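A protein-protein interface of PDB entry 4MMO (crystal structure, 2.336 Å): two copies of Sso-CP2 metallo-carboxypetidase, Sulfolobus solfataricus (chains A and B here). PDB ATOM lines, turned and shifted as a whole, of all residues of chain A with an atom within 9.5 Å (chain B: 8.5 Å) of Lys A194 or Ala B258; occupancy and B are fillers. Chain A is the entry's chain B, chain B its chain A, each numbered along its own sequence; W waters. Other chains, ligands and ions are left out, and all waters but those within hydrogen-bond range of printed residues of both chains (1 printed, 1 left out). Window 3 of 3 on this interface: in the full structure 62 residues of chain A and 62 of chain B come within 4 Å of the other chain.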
ATOM      1  N   ASP A 190       4.624  34.648  -1.154  1.00  0.00           N
ATOM      2  CA  ASP A 190       5.023  33.498  -0.358  1.00  0.00           C
ATOM      3  C   ASP A 190       4.013  33.327   0.768  1.00  0.00           C
ATOM      4  O   ASP A 190       3.984  34.109   1.718  1.00  0.00           O
ATOM      5  CB  ASP A 190       6.441  33.679   0.187  1.00  0.00           C
ATOM      6  CG  ASP A 190       7.100  32.361   0.536  1.00  0.00           C
ATOM      7  OD1 ASP A 190       6.373  31.406   0.882  1.00  0.00           O
ATOM      8  OD2 ASP A 190       8.343  32.275   0.461  1.00  0.00           O
ATOM      9  N   TYR A 191       3.175  32.303   0.642  1.00  0.00           N
ATOM     10  CA  TYR A 191       2.007  32.146   1.502  1.00  0.00           C
ATOM     11  C   TYR A 191       2.211  31.119   2.610  1.00  0.00           C
ATOM     12  O   TYR A 191       1.362  30.973   3.489  1.00  0.00           O
ATOM     13  CB  TYR A 191       0.792  31.746   0.657  1.00  0.00           C
ATOM     14  CG  TYR A 191       0.173  32.871  -0.155  1.00  0.00           C
ATOM     15  CD1 TYR A 191       0.671  34.169  -0.094  1.00  0.00           C
ATOM     16  CD2 TYR A 191      -0.925  32.632  -0.973  1.00  0.00           C
ATOM     17  CE1 TYR A 191       0.095  35.193  -0.830  1.00  0.00           C
ATOM     18  CE2 TYR A 191      -1.505  33.647  -1.711  1.00  0.00           C
ATOM     19  CZ  TYR A 191      -0.991  34.926  -1.636  1.00  0.00           C
ATOM     20  OH  TYR A 191      -1.565  35.943  -2.366  1.00  0.00           O
ATOM     21  N   GLY A 192       3.329  30.405   2.575  1.00  0.00           N
ATOM     22  CA  GLY A 192       3.598  29.401   3.587  1.00  0.00           C
ATOM     23  C   GLY A 192       4.967  28.780   3.431  1.00  0.00           C
ATOM     24  O   GLY A 192       5.729  29.158   2.544  1.00  0.00           O
ATOM     25  N   THR A 193       5.270  27.808   4.285  1.00  0.00           N
ATOM     26  CA  THR A 193       6.595  27.208   4.317  1.00  0.00           C
ATOM     27  C   THR A 193       6.766  26.086   3.296  1.00  0.00           C
ATOM     28  O   THR A 193       7.887  25.797   2.886  1.00  0.00           O
ATOM     29  CB  THR A 193       6.924  26.650   5.718  1.00  0.00           C
ATOM     30  OG1 THR A 193       6.077  25.532   6.005  1.00  0.00           O
ATOM     31  CG2 THR A 193       6.736  27.722   6.784  1.00  0.00           C
ATOM     32  N   LYS A 194       5.668  25.449   2.892  1.00  0.00           N
ATOM     33  CA  LYS A 194       5.756  24.335   1.945  1.00  0.00           C
ATOM     34  C   LYS A 194       4.532  24.197   1.043  1.00  0.00           C
ATOM     35  O   LYS A 194       3.445  24.668   1.368  1.00  0.00           O
ATOM     36  CB  LYS A 194       5.984  23.017   2.693  1.00  0.00           C
ATOM     37  CG  LYS A 194       4.894  22.658   3.697  1.00  0.00           C
ATOM     38  CD  LYS A 194       5.193  21.324   4.375  1.00  0.00           C
ATOM     39  CE  LYS A 194       4.203  21.009   5.486  1.00  0.00           C
ATOM     40  NZ  LYS A 194       2.810  20.852   4.979  1.00  0.00           N
ATOM     41  N   ASP A 195       4.729  23.545  -0.098  1.00  0.00           N
ATOM     42  CA  ASP A 195       3.630  23.216  -0.990  1.00  0.00           C
ATOM     43  C   ASP A 195       2.686  22.260  -0.281  1.00  0.00           C
ATOM     44  O   ASP A 195       3.113  21.426   0.517  1.00  0.00           O
ATOM     45  CB  ASP A 195       4.147  22.554  -2.268  1.00  0.00           C
ATOM     46  CG  ASP A 195       5.147  23.417  -3.017  1.00  0.00           C
ATOM     47  OD1 ASP A 195       5.116  24.657  -2.873  1.00  0.00           O
ATOM     48  OD2 ASP A 195       5.966  22.844  -3.764  1.00  0.00           O
ATOM     49  N   LEU A 196       1.399  22.393  -0.573  1.00  0.00           N
ATOM     50  CA  LEU A 196       0.391  21.518   0.000  1.00  0.00           C
ATOM     51  C   LEU A 196      -0.169  20.647  -1.097  1.00  0.00           C
ATOM     52  O   LEU A 196      -0.131  21.016  -2.270  1.00  0.00           O
ATOM     53  CB  LEU A 196      -0.752  22.330   0.599  1.00  0.00           C
ATOM     54  CG  LEU A 196      -0.359  23.612   1.332  1.00  0.00           C
ATOM     55  CD1 LEU A 196      -1.585  24.467   1.553  1.00  0.00           C
ATOM     56  CD2 LEU A 196       0.322  23.295   2.646  1.00  0.00           C
ATOM     57  N   HIS A 197      -0.695  19.492  -0.719  1.00  0.00           N
ATOM     58  CA  HIS A 197      -1.429  18.689  -1.674  1.00  0.00           C
ATOM     59  C   HIS A 197      -2.670  19.466  -2.101  1.00  0.00           C
ATOM     60  O   HIS A 197      -3.330  20.089  -1.271  1.00  0.00           O
ATOM     61  CB  HIS A 197      -1.837  17.350  -1.077  1.00  0.00           C
ATOM     62  CG  HIS A 197      -2.554  16.470  -2.054  1.00  0.00           C
ATOM     63  ND1 HIS A 197      -3.909  16.272  -2.020  1.00  0.00           N
ATOM     64  CD2 HIS A 197      -2.094  15.805  -3.145  1.00  0.00           C
ATOM     65  CE1 HIS A 197      -4.265  15.484  -3.015  1.00  0.00           C
ATOM     66  NE2 HIS A 197      -3.191  15.190  -3.720  1.00  0.00           N
ATOM     67  N   ASN A 200      -6.216  20.285  -0.509  1.00  0.00           N
ATOM     68  CA  ASN A 200      -6.421  21.342   0.484  1.00  0.00           C
ATOM     69  C   ASN A 200      -6.791  22.695  -0.127  1.00  0.00           C
ATOM     70  O   ASN A 200      -7.012  23.664   0.597  1.00  0.00           O
ATOM     71  CB  ASN A 200      -5.161  21.504   1.333  1.00  0.00           C
ATOM     72  CG  ASN A 200      -4.935  20.334   2.267  1.00  0.00           C
ATOM     73  OD1 ASN A 200      -5.844  19.910   2.979  1.00  0.00           O
ATOM     74  ND2 ASN A 200      -3.721  19.799   2.260  1.00  0.00           N
ATOM     75  N   VAL A 204      -7.230  27.306   1.449  1.00  0.00           N
ATOM     76  CA  VAL A 204      -6.201  28.340   1.355  1.00  0.00           C
ATOM     77  C   VAL A 204      -6.282  29.147   0.063  1.00  0.00           C
ATOM     78  O   VAL A 204      -7.050  28.826  -0.844  1.00  0.00           O
ATOM     79  CB  VAL A 204      -4.788  27.731   1.455  1.00  0.00           C
ATOM     80  CG1 VAL A 204      -4.578  27.107   2.822  1.00  0.00           C
ATOM     81  CG2 VAL A 204      -4.561  26.700   0.353  1.00  0.00           C
ATOM     82  N   ARG A 205      -5.485  30.209  -0.002  1.00  0.00           N
ATOM     83  CA  ARG A 205      -5.335  30.969  -1.230  1.00  0.00           C
ATOM     84  C   ARG A 205      -4.201  30.344  -2.020  1.00  0.00           C
ATOM     85  O   ARG A 205      -3.252  29.810  -1.444  1.00  0.00           O
ATOM     86  CB  ARG A 205      -5.009  32.432  -0.936  1.00  0.00           C
ATOM     87  CG  ARG A 205      -6.074  33.186  -0.156  1.00  0.00           C
ATOM     88  CD  ARG A 205      -5.871  34.689  -0.296  1.00  0.00           C
ATOM     89  NE  ARG A 205      -6.074  35.116  -1.677  1.00  0.00           N
ATOM     90  CZ  ARG A 205      -7.259  35.405  -2.207  1.00  0.00           C
ATOM     91  NH1 ARG A 205      -8.360  35.328  -1.472  1.00  0.00           N
ATOM     92  NH2 ARG A 205      -7.344  35.774  -3.478  1.00  0.00           N
ATOM     93  N   PRO A 207      -1.135  31.120  -4.493  1.00  0.00           N
ATOM     94  CA  PRO A 207      -0.349  32.280  -4.931  1.00  0.00           C
ATOM     95  C   PRO A 207      -0.174  32.387  -6.448  1.00  0.00           C
ATOM     96  O   PRO A 207       0.060  33.495  -6.938  1.00  0.00           O
ATOM     97  CB  PRO A 207       1.006  32.071  -4.245  1.00  0.00           C
ATOM     98  CG  PRO A 207       1.080  30.619  -3.969  1.00  0.00           C
ATOM     99  CD  PRO A 207      -0.326  30.172  -3.709  1.00  0.00           C
ATOM    100  N   ILE A 299      -0.603  19.957  -6.475  1.00  0.00           N
ATOM    101  CA  ILE A 299      -0.252  20.744  -5.296  1.00  0.00           C
ATOM    102  C   ILE A 299      -0.839  22.153  -5.285  1.00  0.00           C
ATOM    103  O   ILE A 299      -1.225  22.692  -6.323  1.00  0.00           O
ATOM    104  CB  ILE A 299       1.284  20.909  -5.174  1.00  0.00           C
ATOM    105  CG1 ILE A 299       1.846  21.662  -6.390  1.00  0.00           C
ATOM    106  CG2 ILE A 299       1.956  19.559  -5.025  1.00  0.00           C
ATOM    107  CD1 ILE A 299       3.344  21.969  -6.301  1.00  0.00           C
ATOM    108  N   VAL A 300      -0.894  22.745  -4.096  1.00  0.00           N
ATOM    109  CA  VAL A 300      -1.017  24.193  -3.970  1.00  0.00           C
ATOM    110  C   VAL A 300       0.383  24.707  -3.659  1.00  0.00           C
ATOM    111  O   VAL A 300       0.900  24.443  -2.572  1.00  0.00           O
ATOM    112  CB  VAL A 300      -1.957  24.612  -2.828  1.00  0.00           C
ATOM    113  CG1 VAL A 300      -2.065  26.137  -2.757  1.00  0.00           C
ATOM    114  CG2 VAL A 300      -3.333  23.982  -3.005  1.00  0.00           C
ATOM    115  N   PRO A 301       1.016  25.424  -4.607  1.00  0.00           N
ATOM    116  CA  PRO A 301       2.362  25.918  -4.289  1.00  0.00           C
ATOM    117  C   PRO A 301       2.321  27.008  -3.223  1.00  0.00           C
ATOM    118  O   PRO A 301       1.297  27.672  -3.074  1.00  0.00           O
ATOM    119  CB  PRO A 301       2.860  26.491  -5.627  1.00  0.00           C
ATOM    120  CG  PRO A 301       1.920  25.952  -6.669  1.00  0.00           C
ATOM    121  CD  PRO A 301       0.606  25.814  -5.967  1.00  0.00           C
ATOM    122  N   HIS A 302       3.410  27.180  -2.483  1.00  0.00           N
ATOM    123  CA  HIS A 302       3.451  28.191  -1.430  1.00  0.00           C
ATOM    124  C   HIS A 302       4.097  29.478  -1.926  1.00  0.00           C
ATOM    125  O   HIS A 302       3.972  30.523  -1.291  1.00  0.00           O
ATOM    126  CB  HIS A 302       4.200  27.666  -0.201  1.00  0.00           C
ATOM    127  CG  HIS A 302       5.681  27.551  -0.394  1.00  0.00           C
ATOM    128  ND1 HIS A 302       6.542  28.605  -0.180  1.00  0.00           N
ATOM    129  CD2 HIS A 302       6.451  26.503  -0.773  1.00  0.00           C
ATOM    130  CE1 HIS A 302       7.783  28.212  -0.422  1.00  0.00           C
ATOM    131  NE2 HIS A 302       7.754  26.944  -0.784  1.00  0.00           N
ATOM    132  N   ARG A 303       4.771  29.398  -3.070  1.00  0.00           N
ATOM    133  CA  ARG A 303       5.555  30.515  -3.580  1.00  0.00           C
ATOM    134  C   ARG A 303       5.321  30.738  -5.071  1.00  0.00           C
ATOM    135  O   ARG A 303       5.169  29.789  -5.837  1.00  0.00           O
ATOM    136  CB  ARG A 303       7.037  30.249  -3.319  1.00  0.00           C
ATOM    137  CG  ARG A 303       7.955  31.429  -3.558  1.00  0.00           C
ATOM    138  CD  ARG A 303       9.321  31.165  -2.935  1.00  0.00           C
ATOM    139  NE  ARG A 303      10.281  32.234  -3.208  1.00  0.00           N
ATOM    140  CZ  ARG A 303      10.446  33.318  -2.454  1.00  0.00           C
ATOM    141  NH1 ARG A 303       9.713  33.507  -1.361  1.00  0.00           N
ATOM    142  NH2 ARG A 303      11.353  34.223  -2.798  1.00  0.00           N
ATOM    143  N   PRO B 169      -5.822  12.198  13.350  1.00  0.00           N
ATOM    144  CA  PRO B 169      -4.890  12.804  14.314  1.00  0.00           C
ATOM    145  C   PRO B 169      -5.103  12.362  15.766  1.00  0.00           C
ATOM    146  O   PRO B 169      -4.144  12.346  16.533  1.00  0.00           O
ATOM    147  CB  PRO B 169      -5.171  14.302  14.173  1.00  0.00           C
ATOM    148  CG  PRO B 169      -5.658  14.458  12.782  1.00  0.00           C
ATOM    149  CD  PRO B 169      -6.454  13.217  12.493  1.00  0.00           C
ATOM    150  N   ASP B 251      -9.047  19.710  14.649  1.00  0.00           N
ATOM    151  CA  ASP B 251      -8.298  20.658  15.463  1.00  0.00           C
ATOM    152  C   ASP B 251      -7.747  21.721  14.519  1.00  0.00           C
ATOM    153  O   ASP B 251      -6.747  21.498  13.838  1.00  0.00           O
ATOM    154  CB  ASP B 251      -7.160  19.954  16.206  1.00  0.00           C
ATOM    155  CG  ASP B 251      -6.467  20.856  17.218  1.00  0.00           C
ATOM    156  OD1 ASP B 251      -6.548  22.094  17.084  1.00  0.00           O
ATOM    157  OD2 ASP B 251      -5.833  20.321  18.150  1.00  0.00           O
ATOM    158  N   VAL B 252      -8.413  22.871  14.480  1.00  0.00           N
ATOM    159  CA  VAL B 252      -8.084  23.927  13.527  1.00  0.00           C
ATOM    160  C   VAL B 252      -6.643  24.407  13.667  1.00  0.00           C
ATOM    161  O   VAL B 252      -5.958  24.619  12.667  1.00  0.00           O
ATOM    162  CB  VAL B 252      -9.038  25.132  13.681  1.00  0.00           C
ATOM    163  CG1 VAL B 252      -8.637  26.272  12.745  1.00  0.00           C
ATOM    164  CG2 VAL B 252     -10.467  24.703  13.407  1.00  0.00           C
ATOM    165  N   GLU B 253      -6.182  24.579  14.902  1.00  0.00           N
ATOM    166  CA  GLU B 253      -4.850  25.120  15.134  1.00  0.00           C
ATOM    167  C   GLU B 253      -3.773  24.097  14.794  1.00  0.00           C
ATOM    168  O   GLU B 253      -2.706  24.453  14.293  1.00  0.00           O
ATOM    169  CB  GLU B 253      -4.695  25.586  16.582  1.00  0.00           C
ATOM    170  CG  GLU B 253      -3.379  26.301  16.862  1.00  0.00           C
ATOM    171  CD  GLU B 253      -3.145  27.486  15.938  1.00  0.00           C
ATOM    172  OE1 GLU B 253      -1.975  27.752  15.589  1.00  0.00           O
ATOM    173  OE2 GLU B 253      -4.134  28.153  15.559  1.00  0.00           O
ATOM    174  N   GLU B 254      -4.053  22.828  15.066  1.00  0.00           N
ATOM    175  CA  GLU B 254      -3.114  21.765  14.738  1.00  0.00           C
ATOM    176  C   GLU B 254      -3.024  21.606  13.222  1.00  0.00           C
ATOM    177  O   GLU B 254      -1.952  21.332  12.676  1.00  0.00           O
ATOM    178  CB  GLU B 254      -3.549  20.448  15.383  1.00  0.00           C
ATOM    179  CG  GLU B 254      -2.413  19.460  15.600  1.00  0.00           C
ATOM    180  CD  GLU B 254      -1.391  19.956  16.609  1.00  0.00           C
ATOM    181  OE1 GLU B 254      -0.198  19.614  16.465  1.00  0.00           O
ATOM    182  OE2 GLU B 254      -1.781  20.683  17.547  1.00  0.00           O
ATOM    183  N   LEU B 255      -4.155  21.787  12.547  1.00  0.00           N
ATOM    184  CA  LEU B 255      -4.208  21.672  11.095  1.00  0.00           C
ATOM    185  C   LEU B 255      -3.451  22.817  10.436  1.00  0.00           C
ATOM    186  O   LEU B 255      -2.676  22.600   9.503  1.00  0.00           O
ATOM    187  CB  LEU B 255      -5.659  21.654  10.605  1.00  0.00           C
ATOM    188  CG  LEU B 255      -5.850  21.654   9.083  1.00  0.00           C
ATOM    189  CD1 LEU B 255      -5.097  20.503   8.428  1.00  0.00           C
ATOM    190  CD2 LEU B 255      -7.325  21.584   8.732  1.00  0.00           C
ATOM    191  N   LYS B 256      -3.673  24.032  10.928  1.00  0.00           N
ATOM    192  CA  LYS B 256      -3.029  25.211  10.368  1.00  0.00           C
ATOM    193  C   LYS B 256      -1.513  25.093  10.451  1.00  0.00           C
ATOM    194  O   LYS B 256      -0.804  25.438   9.506  1.00  0.00           O
ATOM    195  CB  LYS B 256      -3.493  26.477  11.088  1.00  0.00           C
ATOM    196  CG  LYS B 256      -2.835  27.747  10.559  1.00  0.00           C
ATOM    197  CD  LYS B 256      -3.441  29.000  11.170  1.00  0.00           C
ATOM    198  CE  LYS B 256      -2.750  30.251  10.647  1.00  0.00           C
ATOM    199  NZ  LYS B 256      -3.381  31.497  11.158  1.00  0.00           N
ATOM    200  N   LYS B 257      -1.023  24.603  11.584  1.00  0.00           N
ATOM    201  CA  LYS B 257       0.410  24.447  11.788  1.00  0.00           C
ATOM    202  C   LYS B 257       0.970  23.336  10.905  1.00  0.00           C
ATOM    203  O   LYS B 257       2.106  23.419  10.433  1.00  0.00           O
ATOM    204  CB  LYS B 257       0.715  24.148  13.257  1.00  0.00           C
ATOM    205  CG  LYS B 257       2.189  23.902  13.534  1.00  0.00           C
ATOM    206  CD  LYS B 257       2.460  23.686  15.012  1.00  0.00           C
ATOM    207  CE  LYS B 257       3.950  23.521  15.279  1.00  0.00           C
ATOM    208  NZ  LYS B 257       4.574  22.494  14.396  1.00  0.00           N
ATOM    209  N   ALA B 258       0.170  22.298  10.686  1.00  0.00           N
ATOM    210  CA  ALA B 258       0.593  21.172   9.863  1.00  0.00           C
ATOM    211  C   ALA B 258       0.773  21.606   8.410  1.00  0.00           C
ATOM    212  O   ALA B 258       1.766  21.265   7.771  1.00  0.00           O
ATOM    213  CB  ALA B 258      -0.415  20.039   9.959  1.00  0.00           C
ATOM    214  N   LEU B 259      -0.192  22.362   7.897  1.00  0.00           N
ATOM    215  CA  LEU B 259      -0.141  22.839   6.521  1.00  0.00           C
ATOM    216  C   LEU B 259       1.026  23.804   6.326  1.00  0.00           C
ATOM    217  O   LEU B 259       1.777  23.697   5.356  1.00  0.00           O
ATOM    218  CB  LEU B 259      -1.462  23.514   6.147  1.00  0.00           C
ATOM    219  CG  LEU B 259      -2.694  22.607   6.179  1.00  0.00           C
ATOM    220  CD1 LEU B 259      -3.968  23.411   5.938  1.00  0.00           C
ATOM    221  CD2 LEU B 259      -2.572  21.483   5.162  1.00  0.00           C
ATOM    222  N   GLY B 260       1.177  24.744   7.253  1.00  0.00           N
ATOM    223  CA  GLY B 260       2.310  25.653   7.237  1.00  0.00           C
ATOM    224  C   GLY B 260       2.065  26.931   6.458  1.00  0.00           C
ATOM    225  O   GLY B 260       3.007  27.663   6.155  1.00  0.00           O
ATOM    226  N   PHE B 261       0.805  27.196   6.127  1.00  0.00           N
ATOM    227  CA  PHE B 261       0.426  28.448   5.480  1.00  0.00           C
ATOM    228  C   PHE B 261       0.186  29.521   6.537  1.00  0.00           C
ATOM    229  O   PHE B 261      -0.379  29.242   7.596  1.00  0.00           O
ATOM    230  CB  PHE B 261      -0.832  28.263   4.624  1.00  0.00           C
ATOM    231  CG  PHE B 261      -0.551  28.092   3.156  1.00  0.00           C
ATOM    232  CD1 PHE B 261       0.424  27.209   2.719  1.00  0.00           C
ATOM    233  CD2 PHE B 261      -1.274  28.804   2.210  1.00  0.00           C
ATOM    234  CE1 PHE B 261       0.682  27.048   1.365  1.00  0.00           C
ATOM    235  CE2 PHE B 261      -1.020  28.647   0.853  1.00  0.00           C
ATOM    236  CZ  PHE B 261      -0.041  27.766   0.434  1.00  0.00           C
ATOM    237  N   LYS B 262       0.621  30.741   6.239  1.00  0.00           N
ATOM    238  CA  LYS B 262       0.458  31.871   7.148  1.00  0.00           C
ATOM    239  C   LYS B 262      -0.997  32.077   7.559  1.00  0.00           C
ATOM    240  O   LYS B 262      -1.274  32.425   8.706  1.00  0.00           O
ATOM    241  CB  LYS B 262       1.002  33.146   6.498  1.00  0.00           C
ATOM    242  CG  LYS B 262       2.496  33.097   6.226  1.00  0.00           C
ATOM    243  CD  LYS B 262       2.958  34.254   5.354  1.00  0.00           C
ATOM    244  CE  LYS B 262       4.396  34.047   4.897  1.00  0.00           C
ATOM    245  NZ  LYS B 262       4.958  35.241   4.209  1.00  0.00           N
ATOM    246  N   LEU B 264      -5.329  30.673   6.776  1.00  0.00           N
ATOM    247  CA  LEU B 264      -6.343  29.839   6.139  1.00  0.00           C
ATOM    248  C   LEU B 264      -7.538  30.718   5.790  1.00  0.00           C
ATOM    249  O   LEU B 264      -7.682  31.818   6.322  1.00  0.00           O
ATOM    250  CB  LEU B 264      -6.784  28.708   7.071  1.00  0.00           C
ATOM    251  CG  LEU B 264      -5.705  27.731   7.545  1.00  0.00           C
ATOM    252  CD1 LEU B 264      -6.316  26.680   8.460  1.00  0.00           C
ATOM    253  CD2 LEU B 264      -4.998  27.068   6.371  1.00  0.00           C
ATOM    254  N   TYR B 404      -1.803   9.433  11.045  1.00  0.00           N
ATOM    255  CA  TYR B 404      -1.531  10.849  10.822  1.00  0.00           C
ATOM    256  C   TYR B 404      -0.031  11.124  10.875  1.00  0.00           C
ATOM    257  O   TYR B 404       0.469  12.038  10.224  1.00  0.00           O
ATOM    258  CB  TYR B 404      -2.245  11.675  11.893  1.00  0.00           C
ATOM    259  CG  TYR B 404      -2.250  13.167  11.643  1.00  0.00           C
ATOM    260  CD1 TYR B 404      -2.894  13.702  10.536  1.00  0.00           C
ATOM    261  CD2 TYR B 404      -1.631  14.041  12.528  1.00  0.00           C
ATOM    262  CE1 TYR B 404      -2.911  15.066  10.309  1.00  0.00           C
ATOM    263  CE2 TYR B 404      -1.643  15.407  12.310  1.00  0.00           C
ATOM    264  CZ  TYR B 404      -2.285  15.914  11.200  1.00  0.00           C
ATOM    265  OH  TYR B 404      -2.300  17.272  10.980  1.00  0.00           O
ATOM    266  N   ASN B 407       3.424  10.494   7.434  1.00  0.00           N
ATOM    267  CA  ASN B 407       4.125  11.267   6.407  1.00  0.00           C
ATOM    268  C   ASN B 407       4.027  10.633   5.015  1.00  0.00           C
ATOM    269  O   ASN B 407       5.022  10.530   4.293  1.00  0.00           O
ATOM    270  CB  ASN B 407       5.598  11.470   6.791  1.00  0.00           C
ATOM    271  CG  ASN B 407       5.785  12.518   7.874  1.00  0.00           C
ATOM    272  OD1 ASN B 407       5.073  13.522   7.915  1.00  0.00           O
ATOM    273  ND2 ASN B 407       6.752  12.290   8.756  1.00  0.00           N
ATOM    274  N   HIS B 409       3.235  10.624   1.132  1.00  0.00           N
ATOM    275  CA  HIS B 409       3.439  11.680   0.143  1.00  0.00           C
ATOM    276  C   HIS B 409       4.422  12.717   0.682  1.00  0.00           C
ATOM    277  O   HIS B 409       4.269  13.917   0.451  1.00  0.00           O
ATOM    278  N   ALA B 410       5.433  12.237   1.402  1.00  0.00           N
ATOM    279  CA  ALA B 410       6.408  13.105   2.048  1.00  0.00           C
ATOM    280  C   ALA B 410       7.612  12.267   2.472  1.00  0.00           C
ATOM    281  O   ALA B 410       7.531  11.038   2.513  1.00  0.00           O
ATOM    282  CB  ALA B 410       5.778  13.787   3.247  1.00  0.00           C
ATOM    283  N   PRO B 411       8.742  12.920   2.782  1.00  0.00           N
ATOM    284  CA  PRO B 411       9.913  12.118   3.151  1.00  0.00           C
ATOM    285  C   PRO B 411       9.785  11.485   4.533  1.00  0.00           C
ATOM    286  O   PRO B 411       9.046  11.985   5.381  1.00  0.00           O
ATOM    287  CB  PRO B 411      11.056  13.136   3.127  1.00  0.00           C
ATOM    288  CG  PRO B 411      10.406  14.439   3.388  1.00  0.00           C
ATOM    289  CD  PRO B 411       9.051  14.360   2.745  1.00  0.00           C
HETATM  290  O   HOH W   1      -1.021  32.312   3.853  1.00  0.00           O
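The backbone NH of Thr A193 sits at hydrogen-bond distance from the backbone carbonyl oxygen of Gly B260 (2.9 Å).
The backbone NH of Lys B262 sits at hydrogen-bond distance from the backbone carbonyl oxygen of Tyr A191 (2.9 Å).
The backbone carbonyl oxygen of Leu B259 is in hydrogen-bond range of the side-chain amino group of Lys A194 (3.1 Å).
The backbone carbonyl oxygen (O) of Ala B258 sits at hydrogen-bond distance from the side-chain amino group (NZ) of Lys A194, at 3.0 Å.
The side-chain amino group (NZ) of Lys B262 is in hydrogen-bond range of the backbone carbonyl oxygen (O) of Asp A190 (2.9 Å).
The backbone carbonyl oxygen (O) of Leu A196 sits at hydrogen-bond distance from the backbone NH (N) of Val A300, at 2.6 Å.
ND1 of His A302 sits at hydrogen-bond distance from OD1 of Asp A190, at 3.0 Å.
The backbone carbonyl oxygen of Gly A192 is in hydrogen-bond range of a ring nitrogen (ND1) of His A302, at 2.9 Å.
O of Lys B262 lies close to NZ of Lys B256, 3.4 Å away.
The backbone NH of Tyr A191 sits at hydrogen-bond distance from the backbone carbonyl oxygen of His A302.
N of His A302 lies within hydrogen-bond range of OD1 of Asp A195, 3.1 Å away.
Among the printed residues, merely in contact across the chains: Leu A196 with Leu B259 (3.1 Å), Gly A192 with Gly B260 (3.2 Å), Tyr A191 with Phe B261 (3.3 Å), Arg A205 with Phe B261 (3.4 Å), Leu A196 with Phe B261 (3.4 Å), Asn A200 with Leu B259 (3.5 Å), Val A204 with Leu B264 (3.6 Å), Lys A194 with Phe B261 (3.6 Å), Val A204 with Phe B261 (3.8 Å), Pro A301 with Phe B261 (3.8 Å), Gly A192 with Phe B261 (3.8 Å) and His A302 with Phe B261 (3.9 Å).
Of the printed residues of chain B, Leu A196 touches Leu B259 (3.1 Å) and Phe B261 (3.4 Å).
Ala B258 touches just one residue of chain A: Lys A194.
Gly B260 touches two residues of chain A.
Printed residues of chain A within 4 Å of Phe B261: Tyr A191 (3.3 Å), Gly A192 (3.8 Å), Lys A194 (3.6 Å), Leu A196 (3.4 Å), Val A204 (3.8 Å), Arg A205 (3.4 Å), Pro A301 (3.8 Å) and His A302 (3.9 Å).
The nearest printed residue of chain A that does not touch Phe B261 is Val A300 (4.1 Å).
Of the 17 printed residues of chain A, 11 touch a printed residue of chain B.
Printed residues of chain A that touch a printed residue of chain B: Asp A190, Tyr A191, Gly A192, Thr A193, Lys A194, Leu A196, Asn A200, Val A204, Arg A205, Pro A301 and His A302.
Hydrophobic or aromatic side chains of chain B that line the printed part of chain A: Leu B259, Phe B261 and Leu B264.
Among the printed residues, 17 pairs touch across the chains.
No position is printed for both chains.
Water W1 lies within hydrogen-bond range of the backbone carbonyl oxygen (O) of Tyr A191 and the backbone NH (N) of Lys B262.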
